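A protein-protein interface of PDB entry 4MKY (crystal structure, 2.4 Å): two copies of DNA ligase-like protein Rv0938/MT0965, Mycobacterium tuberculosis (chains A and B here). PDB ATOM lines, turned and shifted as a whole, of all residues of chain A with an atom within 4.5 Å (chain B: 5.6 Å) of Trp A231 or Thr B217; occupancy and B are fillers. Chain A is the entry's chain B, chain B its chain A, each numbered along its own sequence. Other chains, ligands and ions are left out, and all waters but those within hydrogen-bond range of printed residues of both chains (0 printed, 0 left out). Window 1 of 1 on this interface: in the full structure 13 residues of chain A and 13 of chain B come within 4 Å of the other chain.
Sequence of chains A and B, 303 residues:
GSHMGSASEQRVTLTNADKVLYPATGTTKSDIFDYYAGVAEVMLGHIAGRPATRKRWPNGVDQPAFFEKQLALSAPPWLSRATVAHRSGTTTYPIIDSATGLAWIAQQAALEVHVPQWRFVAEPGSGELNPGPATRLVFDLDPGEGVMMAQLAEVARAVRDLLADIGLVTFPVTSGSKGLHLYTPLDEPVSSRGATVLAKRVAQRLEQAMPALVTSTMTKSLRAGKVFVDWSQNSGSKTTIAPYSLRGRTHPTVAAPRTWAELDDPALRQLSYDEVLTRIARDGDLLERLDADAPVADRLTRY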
ATOM      1  N   THR A 196     -16.440 -12.948 -22.587  1.00  0.00           N
ATOM      2  CA  THR A 196     -17.391 -11.894 -22.865  1.00  0.00           C
ATOM      3  C   THR A 196     -17.025 -10.583 -22.155  1.00  0.00           C
ATOM      4  O   THR A 196     -17.158  -9.503 -22.732  1.00  0.00           O
ATOM      5  CB  THR A 196     -18.821 -12.333 -22.546  1.00  0.00           C
ATOM      6  OG1 THR A 196     -19.010 -13.674 -23.018  1.00  0.00           O
ATOM      7  CG2 THR A 196     -19.817 -11.396 -23.263  1.00  0.00           C
ATOM      8  N   ALA A 199     -14.201  -9.247 -24.550  1.00  0.00           N
ATOM      9  CA  ALA A 199     -14.648  -8.738 -25.856  1.00  0.00           C
ATOM     10  C   ALA A 199     -15.405  -7.429 -25.631  1.00  0.00           C
ATOM     11  O   ALA A 199     -15.293  -6.468 -26.405  1.00  0.00           O
ATOM     12  CB  ALA A 199     -15.530  -9.778 -26.568  1.00  0.00           C
ATOM     13  N   LYS A 200     -16.071  -7.364 -24.491  1.00  0.00           N
ATOM     14  CA  LYS A 200     -16.792  -6.162 -24.088  1.00  0.00           C
ATOM     15  C   LYS A 200     -15.830  -5.002 -23.750  1.00  0.00           C
ATOM     16  O   LYS A 200     -15.955  -3.921 -24.300  1.00  0.00           O
ATOM     17  CB  LYS A 200     -17.736  -6.480 -22.920  1.00  0.00           C
ATOM     18  CG  LYS A 200     -18.519  -5.272 -22.430  1.00  0.00           C
ATOM     19  CD  LYS A 200     -19.306  -5.576 -21.167  1.00  0.00           C
ATOM     20  CE  LYS A 200     -19.704  -4.297 -20.452  1.00  0.00           C
ATOM     21  NZ  LYS A 200     -20.019  -4.496 -19.020  1.00  0.00           N
ATOM     22  N   ALA A 203     -14.558  -3.737 -27.236  1.00  0.00           N
ATOM     23  CA  ALA A 203     -15.615  -2.980 -27.837  1.00  0.00           C
ATOM     24  C   ALA A 203     -15.715  -1.601 -27.213  1.00  0.00           C
ATOM     25  O   ALA A 203     -15.648  -0.542 -27.899  1.00  0.00           O
ATOM     26  CB  ALA A 203     -16.929  -3.727 -27.647  1.00  0.00           C
ATOM     27  N   SER A 216     -20.713   0.089 -29.482  1.00  0.00           N
ATOM     28  CA  SER A 216     -20.689  -1.231 -28.853  1.00  0.00           C
ATOM     29  C   SER A 216     -22.085  -1.751 -28.526  1.00  0.00           C
ATOM     30  O   SER A 216     -22.228  -2.766 -27.806  1.00  0.00           O
ATOM     31  CB  SER A 216     -19.938  -1.173 -27.539  1.00  0.00           C
ATOM     32  OG  SER A 216     -20.629  -0.279 -26.654  1.00  0.00           O
ATOM     33  N   VAL A 229     -19.768  -3.033 -33.091  1.00  0.00           N
ATOM     34  CA  VAL A 229     -18.836  -4.083 -32.730  1.00  0.00           C
ATOM     35  C   VAL A 229     -19.507  -5.010 -31.723  1.00  0.00           C
ATOM     36  O   VAL A 229     -19.605  -4.723 -30.515  1.00  0.00           O
ATOM     37  CB  VAL A 229     -17.501  -3.526 -32.200  1.00  0.00           C
ATOM     38  CG1 VAL A 229     -16.569  -4.685 -31.837  1.00  0.00           C
ATOM     39  CG2 VAL A 229     -16.857  -2.588 -33.223  1.00  0.00           C
ATOM     40  N   ASP A 230     -20.070  -6.082 -32.234  1.00  0.00           N
ATOM     41  CA  ASP A 230     -20.835  -6.921 -31.378  1.00  0.00           C
ATOM     42  C   ASP A 230     -19.911  -7.908 -30.679  1.00  0.00           C
ATOM     43  O   ASP A 230     -19.301  -8.762 -31.320  1.00  0.00           O
ATOM     44  CB  ASP A 230     -21.881  -7.657 -32.173  1.00  0.00           C
ATOM     45  CG  ASP A 230     -22.879  -8.305 -31.300  1.00  0.00           C
ATOM     46  OD1 ASP A 230     -22.628  -8.370 -30.067  1.00  0.00           O
ATOM     47  OD2 ASP A 230     -23.902  -8.771 -31.843  1.00  0.00           O
ATOM     48  N   TRP A 231     -19.874  -7.811 -29.359  1.00  0.00           N
ATOM     49  CA  TRP A 231     -18.951  -8.574 -28.550  1.00  0.00           C
ATOM     50  C   TRP A 231     -19.740  -9.663 -27.814  1.00  0.00           C
ATOM     51  O   TRP A 231     -19.173 -10.514 -27.161  1.00  0.00           O
ATOM     52  CB  TRP A 231     -18.320  -7.615 -27.538  1.00  0.00           C
ATOM     53  CG  TRP A 231     -19.380  -6.709 -26.972  1.00  0.00           C
ATOM     54  CD1 TRP A 231     -19.850  -5.554 -27.523  1.00  0.00           C
ATOM     55  CD2 TRP A 231     -20.251  -7.009 -25.883  1.00  0.00           C
ATOM     56  NE1 TRP A 231     -20.889  -5.057 -26.780  1.00  0.00           N
ATOM     57  CE2 TRP A 231     -21.177  -5.949 -25.785  1.00  0.00           C
ATOM     58  CE3 TRP A 231     -20.321  -8.060 -24.961  1.00  0.00           C
ATOM     59  CZ2 TRP A 231     -22.165  -5.919 -24.817  1.00  0.00           C
ATOM     60  CZ3 TRP A 231     -21.271  -8.009 -23.971  1.00  0.00           C
ATOM     61  CH2 TRP A 231     -22.202  -6.957 -23.917  1.00  0.00           C
ATOM     62  N   SER A 232     -21.062  -9.626 -27.972  1.00  0.00           N
ATOM     63  CA  SER A 232     -21.978 -10.411 -27.135  1.00  0.00           C
ATOM     64  C   SER A 232     -22.129 -11.874 -27.567  1.00  0.00           C
ATOM     65  O   SER A 232     -22.617 -12.722 -26.795  1.00  0.00           O
ATOM     66  CB  SER A 232     -23.358  -9.761 -27.156  1.00  0.00           C
ATOM     67  OG  SER A 232     -23.929  -9.951 -28.434  1.00  0.00           O
ATOM     68  N   GLN A 233     -21.812 -12.127 -28.838  1.00  0.00           N
ATOM     69  CA  GLN A 233     -21.970 -13.444 -29.400  1.00  0.00           C
ATOM     70  C   GLN A 233     -20.953 -14.395 -28.794  1.00  0.00           C
ATOM     71  O   GLN A 233     -20.964 -15.598 -29.096  1.00  0.00           O
ATOM     72  CB  GLN A 233     -21.826 -13.382 -30.903  1.00  0.00           C
ATOM     73  CG  GLN A 233     -22.972 -12.640 -31.606  1.00  0.00           C
ATOM     74  CD  GLN A 233     -22.722 -12.534 -33.095  1.00  0.00           C
ATOM     75  OE1 GLN A 233     -22.169 -13.452 -33.686  1.00  0.00           O
ATOM     76  NE2 GLN A 233     -23.030 -11.372 -33.690  1.00  0.00           N
ATOM     77  N   ASN A 234     -20.134 -13.867 -27.873  1.00  0.00           N
ATOM     78  CA  ASN A 234     -19.177 -14.659 -27.160  1.00  0.00           C
ATOM     79  C   ASN A 234     -19.894 -15.215 -25.952  1.00  0.00           C
ATOM     80  O   ASN A 234     -19.295 -15.888 -25.079  1.00  0.00           O
ATOM     81  CB  ASN A 234     -18.001 -13.788 -26.718  1.00  0.00           C
ATOM     82  CG  ASN A 234     -17.129 -13.371 -27.865  1.00  0.00           C
ATOM     83  OD1 ASN A 234     -16.284 -14.127 -28.312  1.00  0.00           O
ATOM     84  ND2 ASN A 234     -17.384 -12.201 -28.399  1.00  0.00           N
ATOM     85  N   GLU B 207     -20.345   2.961 -14.981  1.00  0.00           N
ATOM     86  CA  GLU B 207     -19.828   1.593 -14.991  1.00  0.00           C
ATOM     87  C   GLU B 207     -18.323   1.695 -15.023  1.00  0.00           C
ATOM     88  O   GLU B 207     -17.622   1.014 -14.278  1.00  0.00           O
ATOM     89  CB  GLU B 207     -20.361   0.834 -16.223  1.00  0.00           C
ATOM     90  CG  GLU B 207     -19.802  -0.569 -16.424  1.00  0.00           C
ATOM     91  CD  GLU B 207     -20.261  -1.252 -17.712  1.00  0.00           C
ATOM     92  OE1 GLU B 207     -20.216  -0.638 -18.790  1.00  0.00           O
ATOM     93  OE2 GLU B 207     -20.611  -2.453 -17.651  1.00  0.00           O
ATOM     94  N   THR B 215     -23.169  -2.501 -13.987  1.00  0.00           N
ATOM     95  CA  THR B 215     -23.023  -2.893 -15.393  1.00  0.00           C
ATOM     96  C   THR B 215     -23.957  -2.062 -16.290  1.00  0.00           C
ATOM     97  O   THR B 215     -25.015  -1.653 -15.837  1.00  0.00           O
ATOM     98  CB  THR B 215     -23.255  -4.409 -15.648  1.00  0.00           C
ATOM     99  OG1 THR B 215     -23.049  -4.690 -17.050  1.00  0.00           O
ATOM    100  CG2 THR B 215     -24.691  -4.860 -15.249  1.00  0.00           C
ATOM    101  N   SER B 216     -23.600  -1.872 -17.562  1.00  0.00           N
ATOM    102  CA  SER B 216     -24.451  -1.103 -18.492  1.00  0.00           C
ATOM    103  C   SER B 216     -25.056  -1.968 -19.593  1.00  0.00           C
ATOM    104  O   SER B 216     -25.876  -1.487 -20.400  1.00  0.00           O
ATOM    105  CB  SER B 216     -23.659   0.021 -19.152  1.00  0.00           C
ATOM    106  OG  SER B 216     -22.541  -0.518 -19.858  1.00  0.00           O
ATOM    107  N   THR B 217     -24.704  -3.257 -19.590  1.00  0.00           N
ATOM    108  CA  THR B 217     -25.191  -4.208 -20.586  1.00  0.00           C
ATOM    109  C   THR B 217     -26.154  -5.216 -19.984  1.00  0.00           C
ATOM    110  O   THR B 217     -26.163  -5.444 -18.762  1.00  0.00           O
ATOM    111  CB  THR B 217     -24.028  -4.971 -21.226  1.00  0.00           C
ATOM    112  OG1 THR B 217     -23.273  -5.634 -20.206  1.00  0.00           O
ATOM    113  CG2 THR B 217     -23.099  -4.006 -21.921  1.00  0.00           C
ATOM    114  N   MET B 218     -26.945  -5.858 -20.838  1.00  0.00           N
ATOM    115  CA  MET B 218     -27.945  -6.812 -20.402  1.00  0.00           C
ATOM    116  C   MET B 218     -27.354  -8.161 -20.057  1.00  0.00           C
ATOM    117  O   MET B 218     -27.971  -8.915 -19.324  1.00  0.00           O
ATOM    118  CB  MET B 218     -28.897  -7.107 -21.538  1.00  0.00           C
ATOM    119  CG  MET B 218     -30.053  -6.169 -21.795  1.00  0.00           C
ATOM    120  SD  MET B 218     -30.926  -6.971 -23.169  1.00  0.00           S
ATOM    121  CE  MET B 218     -29.550  -7.464 -24.209  1.00  0.00           C
ATOM    122  N   THR B 219     -26.255  -8.541 -20.708  1.00  0.00           N
ATOM    123  CA  THR B 219     -25.804  -9.933 -20.648  1.00  0.00           C
ATOM    124  C   THR B 219     -26.006 -10.535 -19.271  1.00  0.00           C
ATOM    125  O   THR B 219     -25.252 -10.228 -18.361  1.00  0.00           O
ATOM    126  CB  THR B 219     -24.313 -10.069 -20.994  1.00  0.00           C
ATOM    127  OG1 THR B 219     -24.000  -9.173 -22.062  1.00  0.00           O
ATOM    128  CG2 THR B 219     -24.018 -11.470 -21.442  1.00  0.00           C
ATOM    129  N   LEU B 222     -23.213 -11.575 -16.906  1.00  0.00           N
ATOM    130  CA  LEU B 222     -22.371 -10.523 -16.372  1.00  0.00           C
ATOM    131  C   LEU B 222     -23.130  -9.773 -15.312  1.00  0.00           C
ATOM    132  O   LEU B 222     -22.638  -8.785 -14.752  1.00  0.00           O
ATOM    133  CB  LEU B 222     -21.999  -9.535 -17.477  1.00  0.00           C
ATOM    134  CG  LEU B 222     -21.029  -9.937 -18.588  1.00  0.00           C
ATOM    135  CD1 LEU B 222     -20.789  -8.759 -19.522  1.00  0.00           C
ATOM    136  CD2 LEU B 222     -19.723 -10.413 -17.984  1.00  0.00           C
ATOM    137  N   ARG B 223     -24.389 -10.138 -15.130  1.00  0.00           N
ATOM    138  CA  ARG B 223     -25.255  -9.321 -14.300  1.00  0.00           C
ATOM    139  C   ARG B 223     -25.013  -9.556 -12.817  1.00  0.00           C
ATOM    140  O   ARG B 223     -25.405  -8.748 -11.997  1.00  0.00           O
ATOM    141  CB  ARG B 223     -26.719  -9.619 -14.624  1.00  0.00           C
ATOM    142  CG  ARG B 223     -27.154  -9.255 -16.041  1.00  0.00           C
ATOM    143  CD  ARG B 223     -27.735  -7.842 -16.118  1.00  0.00           C
ATOM    144  NE  ARG B 223     -29.096  -7.906 -16.622  1.00  0.00           N
ATOM    145  CZ  ARG B 223     -30.155  -8.063 -15.839  1.00  0.00           C
ATOM    146  NH1 ARG B 223     -29.990  -8.112 -14.525  1.00  0.00           N
ATOM    147  NH2 ARG B 223     -31.373  -8.157 -16.342  1.00  0.00           N
ATOM    148  N   PHE B 228     -27.603  -3.570 -12.871  1.00  0.00           N
ATOM    149  CA  PHE B 228     -27.759  -3.211 -14.292  1.00  0.00           C
ATOM    150  C   PHE B 228     -28.469  -1.858 -14.384  1.00  0.00           C
ATOM    151  O   PHE B 228     -29.648  -1.725 -14.021  1.00  0.00           O
ATOM    152  CB  PHE B 228     -28.521  -4.292 -15.037  1.00  0.00           C
ATOM    153  CG  PHE B 228     -28.928  -3.930 -16.448  1.00  0.00           C
ATOM    154  CD1 PHE B 228     -28.021  -3.341 -17.333  1.00  0.00           C
ATOM    155  CD2 PHE B 228     -30.133  -4.398 -16.965  1.00  0.00           C
ATOM    156  CE1 PHE B 228     -28.387  -3.039 -18.623  1.00  0.00           C
ATOM    157  CE2 PHE B 228     -30.476  -4.153 -18.295  1.00  0.00           C
ATOM    158  CZ  PHE B 228     -29.636  -3.402 -19.083  1.00  0.00           C
ATOM    159  N   TRP B 231     -30.396   1.763 -19.478  1.00  0.00           N
ATOM    160  CA  TRP B 231     -30.487   3.075 -20.080  1.00  0.00           C
ATOM    161  C   TRP B 231     -31.340   2.941 -21.332  1.00  0.00           C
ATOM    162  O   TRP B 231     -31.774   3.922 -21.935  1.00  0.00           O
ATOM    163  CB  TRP B 231     -29.068   3.545 -20.449  1.00  0.00           C
ATOM    164  CG  TRP B 231     -28.285   2.518 -21.186  1.00  0.00           C
ATOM    165  CD1 TRP B 231     -27.476   1.595 -20.645  1.00  0.00           C
ATOM    166  CD2 TRP B 231     -28.323   2.231 -22.620  1.00  0.00           C
ATOM    167  NE1 TRP B 231     -27.031   0.715 -21.619  1.00  0.00           N
ATOM    168  CE2 TRP B 231     -27.517   1.100 -22.839  1.00  0.00           C
ATOM    169  CE3 TRP B 231     -28.967   2.824 -23.714  1.00  0.00           C
ATOM    170  CZ2 TRP B 231     -27.381   0.493 -24.105  1.00  0.00           C
ATOM    171  CZ3 TRP B 231     -28.808   2.257 -24.983  1.00  0.00           C
ATOM    172  CH2 TRP B 231     -28.024   1.096 -25.165  1.00  0.00           C
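Among the printed residues, pairs that only touch across the chains: Trp A231 with Thr B219 (3.4 Å), Trp A231 with Thr B217 (3.6 Å), Lys A200 with Thr B215 (3.6 Å), Lys A200 with Thr B217 (3.6 Å) and Lys A200 with Leu B222 (3.9 Å).
The side-chain carboxylate (OE1) of Glu B207 is in hydrogen-bond range of the side-chain hydroxyl (OG) of Ser B216, 2.6 Å away.
ND2 of Asn A234 lies within hydrogen-bond range of O of Trp A231.
The side-chain hydroxyl (OG1) of Thr B215 is in hydrogen-bond range of the side-chain hydroxyl (OG1) of Thr B217 (3.3 Å).
The side-chain carboxylate (OE2) of Glu B207 lies close to the side-chain hydroxyl (OG1) of Thr B215, at 3.4 Å.
The backbone carbonyl oxygen (O) of Ser A216 is in hydrogen-bond range of the indole nitrogen (NE1) of Trp A231, at 2.8 Å.
Of the 11 printed residues of chain A, 2 touch a printed residue of chain B.
Among the printed residues, 6 pairs touch across the chains.
Among the printed residues, Asp or Glu carboxylates within 4 Å of a Lys or Arg side-chain nitrogen of the other chain: Lys A200 with Glu B207 (2.5 Å).
Of the printed residues of chain B, Lys A200 touches Glu B207, Thr B215, Thr B217 and Leu B222.
Ala A203 touches none of the printed residues of chain B.
Trp A231 touches just these residues of chain B: Thr B217 and Thr B219.
Printed residues of chain A within 4 Å of Thr B215: Lys A200.
Thr B217 touches just these residues of chain A: Lys A200 (3.6 Å) and Trp A231 (3.6 Å).
Met B218 touches none of the printed residues of chain A.
The nearest residue of chain B that does not touch Trp A231 is Leu B222 (4.5 Å).
Positions printed for both chains: 216 and 231.
NZ of Lys A200 lies within salt-bridge range of OE2 of Glu B207 (2.5 Å).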
